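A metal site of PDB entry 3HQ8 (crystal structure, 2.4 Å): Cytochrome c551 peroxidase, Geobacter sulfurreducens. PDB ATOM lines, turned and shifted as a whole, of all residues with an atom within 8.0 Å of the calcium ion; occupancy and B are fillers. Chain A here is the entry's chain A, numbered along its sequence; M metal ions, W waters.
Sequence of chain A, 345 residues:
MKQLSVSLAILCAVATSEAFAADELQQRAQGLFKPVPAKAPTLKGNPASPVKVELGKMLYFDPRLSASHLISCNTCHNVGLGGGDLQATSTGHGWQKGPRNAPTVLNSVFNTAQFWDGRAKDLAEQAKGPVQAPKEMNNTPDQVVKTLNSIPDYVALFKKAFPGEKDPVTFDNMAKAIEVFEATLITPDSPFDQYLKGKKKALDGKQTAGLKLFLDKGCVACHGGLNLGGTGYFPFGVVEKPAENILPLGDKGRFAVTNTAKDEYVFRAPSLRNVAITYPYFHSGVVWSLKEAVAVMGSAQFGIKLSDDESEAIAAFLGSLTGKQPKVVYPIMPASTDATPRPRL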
ATOM      1  N   GLY A  84     -13.680 -20.741  27.603  1.00  0.00           N
ATOM      2  CA  GLY A  84     -12.578 -21.400  28.291  1.00  0.00           C
ATOM      3  C   GLY A  84     -12.975 -21.819  29.676  1.00  0.00           C
ATOM      4  O   GLY A  84     -14.094 -22.306  29.865  1.00  0.00           O
ATOM      5  N   ASP A  85     -12.074 -21.645  30.653  1.00  0.00           N
ATOM      6  CA  ASP A  85     -12.326 -22.147  32.018  1.00  0.00           C
ATOM      7  C   ASP A  85     -11.842 -21.213  33.160  1.00  0.00           C
ATOM      8  O   ASP A  85     -11.799 -21.624  34.336  1.00  0.00           O
ATOM      9  CB  ASP A  85     -11.745 -23.581  32.157  1.00  0.00           C
ATOM     10  CG  ASP A  85     -10.205 -23.613  32.423  1.00  0.00           C
ATOM     11  OD1 ASP A  85      -9.515 -22.559  32.320  1.00  0.00           O
ATOM     12  OD2 ASP A  85      -9.694 -24.716  32.744  1.00  0.00           O
ATOM     13  N   LEU A  86     -11.486 -19.984  32.798  1.00  0.00           N
ATOM     14  CA  LEU A  86     -10.889 -18.996  33.707  1.00  0.00           C
ATOM     15  C   LEU A  86      -9.772 -19.558  34.623  1.00  0.00           C
ATOM     16  O   LEU A  86      -9.570 -19.055  35.729  1.00  0.00           O
ATOM     17  CB  LEU A  86     -11.968 -18.326  34.572  1.00  0.00           C
ATOM     18  CG  LEU A  86     -13.380 -18.047  34.042  1.00  0.00           C
ATOM     19  CD1 LEU A  86     -14.355 -18.055  35.198  1.00  0.00           C
ATOM     20  CD2 LEU A  86     -13.499 -16.756  33.210  1.00  0.00           C
ATOM     21  N   GLN A  87      -9.090 -20.601  34.186  1.00  0.00           N
ATOM     22  CA  GLN A  87      -7.963 -21.175  34.955  1.00  0.00           C
ATOM     23  C   GLN A  87      -6.668 -20.976  34.207  1.00  0.00           C
ATOM     24  O   GLN A  87      -6.654 -20.869  32.972  1.00  0.00           O
ATOM     25  CB  GLN A  87      -8.136 -22.669  35.230  1.00  0.00           C
ATOM     26  CG  GLN A  87      -9.412 -23.066  35.952  1.00  0.00           C
ATOM     27  CD  GLN A  87      -9.497 -22.595  37.383  1.00  0.00           C
ATOM     28  OE1 GLN A  87      -8.606 -22.835  38.214  1.00  0.00           O
ATOM     29  NE2 GLN A  87     -10.574 -21.943  37.703  1.00  0.00           N
ATOM     30  N   ALA A  88      -5.580 -20.924  34.987  1.00  0.00           N
ATOM     31  CA  ALA A  88      -4.244 -20.770  34.454  1.00  0.00           C
ATOM     32  C   ALA A  88      -4.009 -22.014  33.614  1.00  0.00           C
ATOM     33  O   ALA A  88      -3.728 -21.944  32.431  1.00  0.00           O
ATOM     34  CB  ALA A  88      -3.226 -20.662  35.589  1.00  0.00           C
ATOM     35  N   ASN A 101      -3.469 -24.285  29.522  1.00  0.00           N
ATOM     36  CA  ASN A 101      -4.687 -23.488  29.362  1.00  0.00           C
ATOM     37  C   ASN A 101      -5.753 -24.226  28.541  1.00  0.00           C
ATOM     38  O   ASN A 101      -5.430 -24.772  27.508  1.00  0.00           O
ATOM     39  CB  ASN A 101      -4.350 -22.157  28.676  1.00  0.00           C
ATOM     40  CG  ASN A 101      -5.201 -21.039  29.180  1.00  0.00           C
ATOM     41  OD1 ASN A 101      -5.849 -20.322  28.385  1.00  0.00           O
ATOM     42  ND2 ASN A 101      -5.234 -20.839  30.506  1.00  0.00           N
ATOM     43  N   ALA A 102      -6.995 -24.303  29.023  1.00  0.00           N
ATOM     44  CA  ALA A 102      -8.135 -24.665  28.147  1.00  0.00           C
ATOM     45  C   ALA A 102      -8.344 -23.528  27.149  1.00  0.00           C
ATOM     46  O   ALA A 102      -8.818 -22.461  27.522  1.00  0.00           O
ATOM     47  CB  ALA A 102      -9.444 -24.937  28.941  1.00  0.00           C
ATOM     48  N   PRO A 103      -7.912 -23.716  25.895  1.00  0.00           N
ATOM     49  CA  PRO A 103      -8.099 -22.704  24.835  1.00  0.00           C
ATOM     50  C   PRO A 103      -9.594 -22.533  24.695  1.00  0.00           C
ATOM     51  O   PRO A 103     -10.292 -23.458  25.076  1.00  0.00           O
ATOM     52  CB  PRO A 103      -7.546 -23.415  23.589  1.00  0.00           C
ATOM     53  CG  PRO A 103      -7.917 -24.842  23.836  1.00  0.00           C
ATOM     54  CD  PRO A 103      -7.588 -25.032  25.332  1.00  0.00           C
ATOM     55  N   THR A 104     -10.075 -21.397  24.187  1.00  0.00           N
ATOM     56  CA  THR A 104     -11.558 -21.221  23.954  1.00  0.00           C
ATOM     57  C   THR A 104     -12.128 -22.329  23.115  1.00  0.00           C
ATOM     58  O   THR A 104     -11.393 -23.082  22.553  1.00  0.00           O
ATOM     59  CB  THR A 104     -11.928 -19.848  23.331  1.00  0.00           C
ATOM     60  OG1 THR A 104     -13.354 -19.643  23.457  1.00  0.00           O
ATOM     61  CG2 THR A 104     -11.512 -19.758  21.865  1.00  0.00           C
ATOM     62  N   TRP A 116      -1.396 -27.200  21.349  1.00  0.00           N
ATOM     63  CA  TRP A 116      -0.665 -26.029  21.778  1.00  0.00           C
ATOM     64  C   TRP A 116       0.764 -26.118  21.311  1.00  0.00           C
ATOM     65  O   TRP A 116       1.328 -25.127  20.868  1.00  0.00           O
ATOM     66  CB  TRP A 116      -0.667 -25.950  23.294  1.00  0.00           C
ATOM     67  CG  TRP A 116      -1.697 -25.029  23.871  1.00  0.00           C
ATOM     68  CD1 TRP A 116      -2.827 -25.378  24.534  1.00  0.00           C
ATOM     69  CD2 TRP A 116      -1.652 -23.592  23.896  1.00  0.00           C
ATOM     70  NE1 TRP A 116      -3.510 -24.268  24.939  1.00  0.00           N
ATOM     71  CE2 TRP A 116      -2.804 -23.147  24.571  1.00  0.00           C
ATOM     72  CE3 TRP A 116      -0.747 -22.633  23.397  1.00  0.00           C
ATOM     73  CZ2 TRP A 116      -3.097 -21.806  24.770  1.00  0.00           C
ATOM     74  CZ3 TRP A 116      -1.038 -21.287  23.608  1.00  0.00           C
ATOM     75  CH2 TRP A 116      -2.197 -20.891  24.285  1.00  0.00           C
ATOM     76  N   PRO A 270      -2.018 -18.969  18.602  1.00  0.00           N
ATOM     77  CA  PRO A 270      -3.440 -19.126  18.832  1.00  0.00           C
ATOM     78  C   PRO A 270      -4.221 -18.080  18.085  1.00  0.00           C
ATOM     79  O   PRO A 270      -3.683 -17.024  17.741  1.00  0.00           O
ATOM     80  CB  PRO A 270      -3.597 -18.820  20.338  1.00  0.00           C
ATOM     81  CG  PRO A 270      -2.224 -18.801  20.895  1.00  0.00           C
ATOM     82  CD  PRO A 270      -1.385 -18.320  19.766  1.00  0.00           C
ATOM     83  N   VAL A 275      -9.979 -12.652  22.253  1.00  0.00           N
ATOM     84  CA  VAL A 275      -8.881 -12.769  23.209  1.00  0.00           C
ATOM     85  C   VAL A 275      -9.149 -11.973  24.477  1.00  0.00           C
ATOM     86  O   VAL A 275      -8.707 -12.372  25.535  1.00  0.00           O
ATOM     87  CB  VAL A 275      -7.507 -12.358  22.616  1.00  0.00           C
ATOM     88  CG1 VAL A 275      -7.473 -10.887  22.261  1.00  0.00           C
ATOM     89  CG2 VAL A 275      -6.381 -12.697  23.589  1.00  0.00           C
ATOM     90  N   ILE A 277     -11.774 -11.754  26.303  1.00  0.00           N
ATOM     91  CA  ILE A 277     -12.588 -12.495  27.285  1.00  0.00           C
ATOM     92  C   ILE A 277     -12.077 -13.884  27.737  1.00  0.00           C
ATOM     93  O   ILE A 277     -12.741 -14.502  28.583  1.00  0.00           O
ATOM     94  CB  ILE A 277     -14.101 -12.576  26.888  1.00  0.00           C
ATOM     95  CG1 ILE A 277     -14.315 -13.311  25.564  1.00  0.00           C
ATOM     96  CG2 ILE A 277     -14.728 -11.168  26.856  1.00  0.00           C
ATOM     97  CD1 ILE A 277     -15.782 -13.400  25.165  1.00  0.00           C
ATOM     98  N   THR A 278     -10.907 -14.326  27.208  1.00  0.00           N
ATOM     99  CA  THR A 278     -10.270 -15.640  27.527  1.00  0.00           C
ATOM    100  C   THR A 278      -8.947 -15.673  28.354  1.00  0.00           C
ATOM    101  O   THR A 278      -8.225 -16.673  28.373  1.00  0.00           O
ATOM    102  CB  THR A 278     -10.035 -16.477  26.244  1.00  0.00           C
ATOM    103  OG1 THR A 278      -8.726 -16.159  25.714  1.00  0.00           O
ATOM    104  CG2 THR A 278     -11.179 -16.235  25.155  1.00  0.00           C
ATOM    105  N   TYR A 279      -8.597 -14.580  29.026  1.00  0.00           N
ATOM    106  CA  TYR A 279      -7.606 -14.588  30.118  1.00  0.00           C
ATOM    107  C   TYR A 279      -7.668 -15.892  30.951  1.00  0.00           C
ATOM    108  O   TYR A 279      -8.730 -16.519  31.073  1.00  0.00           O
ATOM    109  CB  TYR A 279      -7.862 -13.392  31.039  1.00  0.00           C
ATOM    110  CG  TYR A 279      -9.282 -13.366  31.600  1.00  0.00           C
ATOM    111  CD1 TYR A 279      -9.564 -13.936  32.836  1.00  0.00           C
ATOM    112  CD2 TYR A 279     -10.350 -12.839  30.853  1.00  0.00           C
ATOM    113  CE1 TYR A 279     -10.877 -13.975  33.334  1.00  0.00           C
ATOM    114  CE2 TYR A 279     -11.663 -12.864  31.352  1.00  0.00           C
ATOM    115  CZ  TYR A 279     -11.922 -13.428  32.582  1.00  0.00           C
ATOM    116  OH  TYR A 279     -13.211 -13.454  33.086  1.00  0.00           O
ATOM    117  N   PRO A 280      -6.532 -16.305  31.553  1.00  0.00           N
ATOM    118  CA  PRO A 280      -5.200 -15.751  31.381  1.00  0.00           C
ATOM    119  C   PRO A 280      -4.583 -16.305  30.081  1.00  0.00           C
ATOM    120  O   PRO A 280      -5.228 -17.086  29.387  1.00  0.00           O
ATOM    121  CB  PRO A 280      -4.435 -16.220  32.626  1.00  0.00           C
ATOM    122  CG  PRO A 280      -5.159 -17.380  33.142  1.00  0.00           C
ATOM    123  CD  PRO A 280      -6.598 -17.267  32.672  1.00  0.00           C
ATOM    124  N   TYR A 281      -3.336 -15.923  29.790  1.00  0.00           N
ATOM    125  CA  TYR A 281      -2.830 -16.070  28.419  1.00  0.00           C
ATOM    126  C   TYR A 281      -1.653 -16.965  28.268  1.00  0.00           C
ATOM    127  O   TYR A 281      -0.932 -17.251  29.248  1.00  0.00           O
ATOM    128  CB  TYR A 281      -2.532 -14.694  27.827  1.00  0.00           C
ATOM    129  CG  TYR A 281      -3.786 -13.898  27.713  1.00  0.00           C
ATOM    130  CD1 TYR A 281      -4.733 -14.256  26.745  1.00  0.00           C
ATOM    131  CD2 TYR A 281      -4.053 -12.840  28.575  1.00  0.00           C
ATOM    132  CE1 TYR A 281      -5.916 -13.562  26.622  1.00  0.00           C
ATOM    133  CE2 TYR A 281      -5.250 -12.147  28.479  1.00  0.00           C
ATOM    134  CZ  TYR A 281      -6.181 -12.516  27.467  1.00  0.00           C
ATOM    135  OH  TYR A 281      -7.352 -11.841  27.304  1.00  0.00           O
ATOM    136  N   PHE A 282      -1.487 -17.396  27.011  1.00  0.00           N
ATOM    137  CA  PHE A 282      -0.416 -18.308  26.574  1.00  0.00           C
ATOM    138  C   PHE A 282      -0.744 -19.727  26.985  1.00  0.00           C
ATOM    139  O   PHE A 282      -1.797 -19.968  27.576  1.00  0.00           O
ATOM    140  CB  PHE A 282       0.969 -17.844  27.048  1.00  0.00           C
ATOM    141  CG  PHE A 282       1.328 -16.464  26.564  1.00  0.00           C
ATOM    142  CD1 PHE A 282       1.286 -16.146  25.187  1.00  0.00           C
ATOM    143  CD2 PHE A 282       1.656 -15.470  27.461  1.00  0.00           C
ATOM    144  CE1 PHE A 282       1.597 -14.879  24.734  1.00  0.00           C
ATOM    145  CE2 PHE A 282       1.960 -14.189  27.002  1.00  0.00           C
ATOM    146  CZ  PHE A 282       1.937 -13.901  25.645  1.00  0.00           C
ATOM    147  N   HIS A 283       0.144 -20.672  26.629  1.00  0.00           N
ATOM    148  CA  HIS A 283      -0.081 -22.117  26.848  1.00  0.00           C
ATOM    149  C   HIS A 283      -0.115 -22.482  28.330  1.00  0.00           C
ATOM    150  O   HIS A 283      -0.651 -23.521  28.729  1.00  0.00           O
ATOM    151  CB  HIS A 283       0.982 -22.950  26.088  1.00  0.00           C
ATOM    152  CG  HIS A 283       2.347 -22.878  26.700  1.00  0.00           C
ATOM    153  ND1 HIS A 283       3.234 -21.862  26.414  1.00  0.00           N
ATOM    154  CD2 HIS A 283       2.958 -23.685  27.600  1.00  0.00           C
ATOM    155  CE1 HIS A 283       4.344 -22.054  27.119  1.00  0.00           C
ATOM    156  NE2 HIS A 283       4.195 -23.148  27.838  1.00  0.00           N
ATOM    157  N   SER A 284       0.473 -21.644  29.163  1.00  0.00           N
ATOM    158  CA  SER A 284       0.627 -22.019  30.568  1.00  0.00           C
ATOM    159  C   SER A 284      -0.311 -21.176  31.392  1.00  0.00           C
ATOM    160  O   SER A 284      -0.480 -21.408  32.591  1.00  0.00           O
ATOM    161  CB  SER A 284       2.079 -21.839  31.004  1.00  0.00           C
ATOM    162  OG  SER A 284       2.629 -20.705  30.359  1.00  0.00           O
ATOM    163  N   GLY A 285      -0.934 -20.206  30.724  1.00  0.00           N
ATOM    164  CA  GLY A 285      -1.800 -19.234  31.388  1.00  0.00           C
ATOM    165  C   GLY A 285      -1.124 -18.426  32.477  1.00  0.00           C
ATOM    166  O   GLY A 285      -1.756 -18.127  33.491  1.00  0.00           O
ATOM    167  N   VAL A 287       0.123 -15.288  32.155  1.00  0.00           N
ATOM    168  CA  VAL A 287      -0.040 -13.837  32.004  1.00  0.00           C
ATOM    169  C   VAL A 287      -1.522 -13.429  31.904  1.00  0.00           C
ATOM    170  O   VAL A 287      -2.148 -13.589  30.842  1.00  0.00           O
ATOM    171  CB  VAL A 287       0.764 -13.334  30.773  1.00  0.00           C
ATOM    172  CG1 VAL A 287       0.353 -11.924  30.368  1.00  0.00           C
ATOM    173  CG2 VAL A 287       2.243 -13.358  31.067  1.00  0.00           C
HETATM  174 CA    CA M   1      -6.504 -18.294  27.713  1.00  0.00          CA
HETATM  175  O   HOH W   1      -7.635 -20.245  26.816  1.00  0.00           O
HETATM  176  O   HOH W   2      -4.973 -18.442  26.293  1.00  0.00           O
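O of Asn 101 is in hydrogen-bond range of NE1 of Trp 116. O of Gln 87 sits at hydrogen-bond distance from ND2 of Asn 101, 2.8 Å away. ND2 of Asn 101 sits at hydrogen-bond distance from O of Ala 88. The backbone carbonyl oxygen of His 283 is in hydrogen-bond range of the backbone NH of Asn 101.
Water W2 binds the calcium ion, 2.1 Å away. The side-chain amide oxygen (OD1) of Asn 101 binds the calcium ion (2.2 Å). The calcium ion is bound by the backbone carbonyl oxygen (O) of Pro 280 (2.4 Å). Water W1 binds the calcium ion. O of Thr 278 is bound to the calcium ion, at 2.5 Å.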
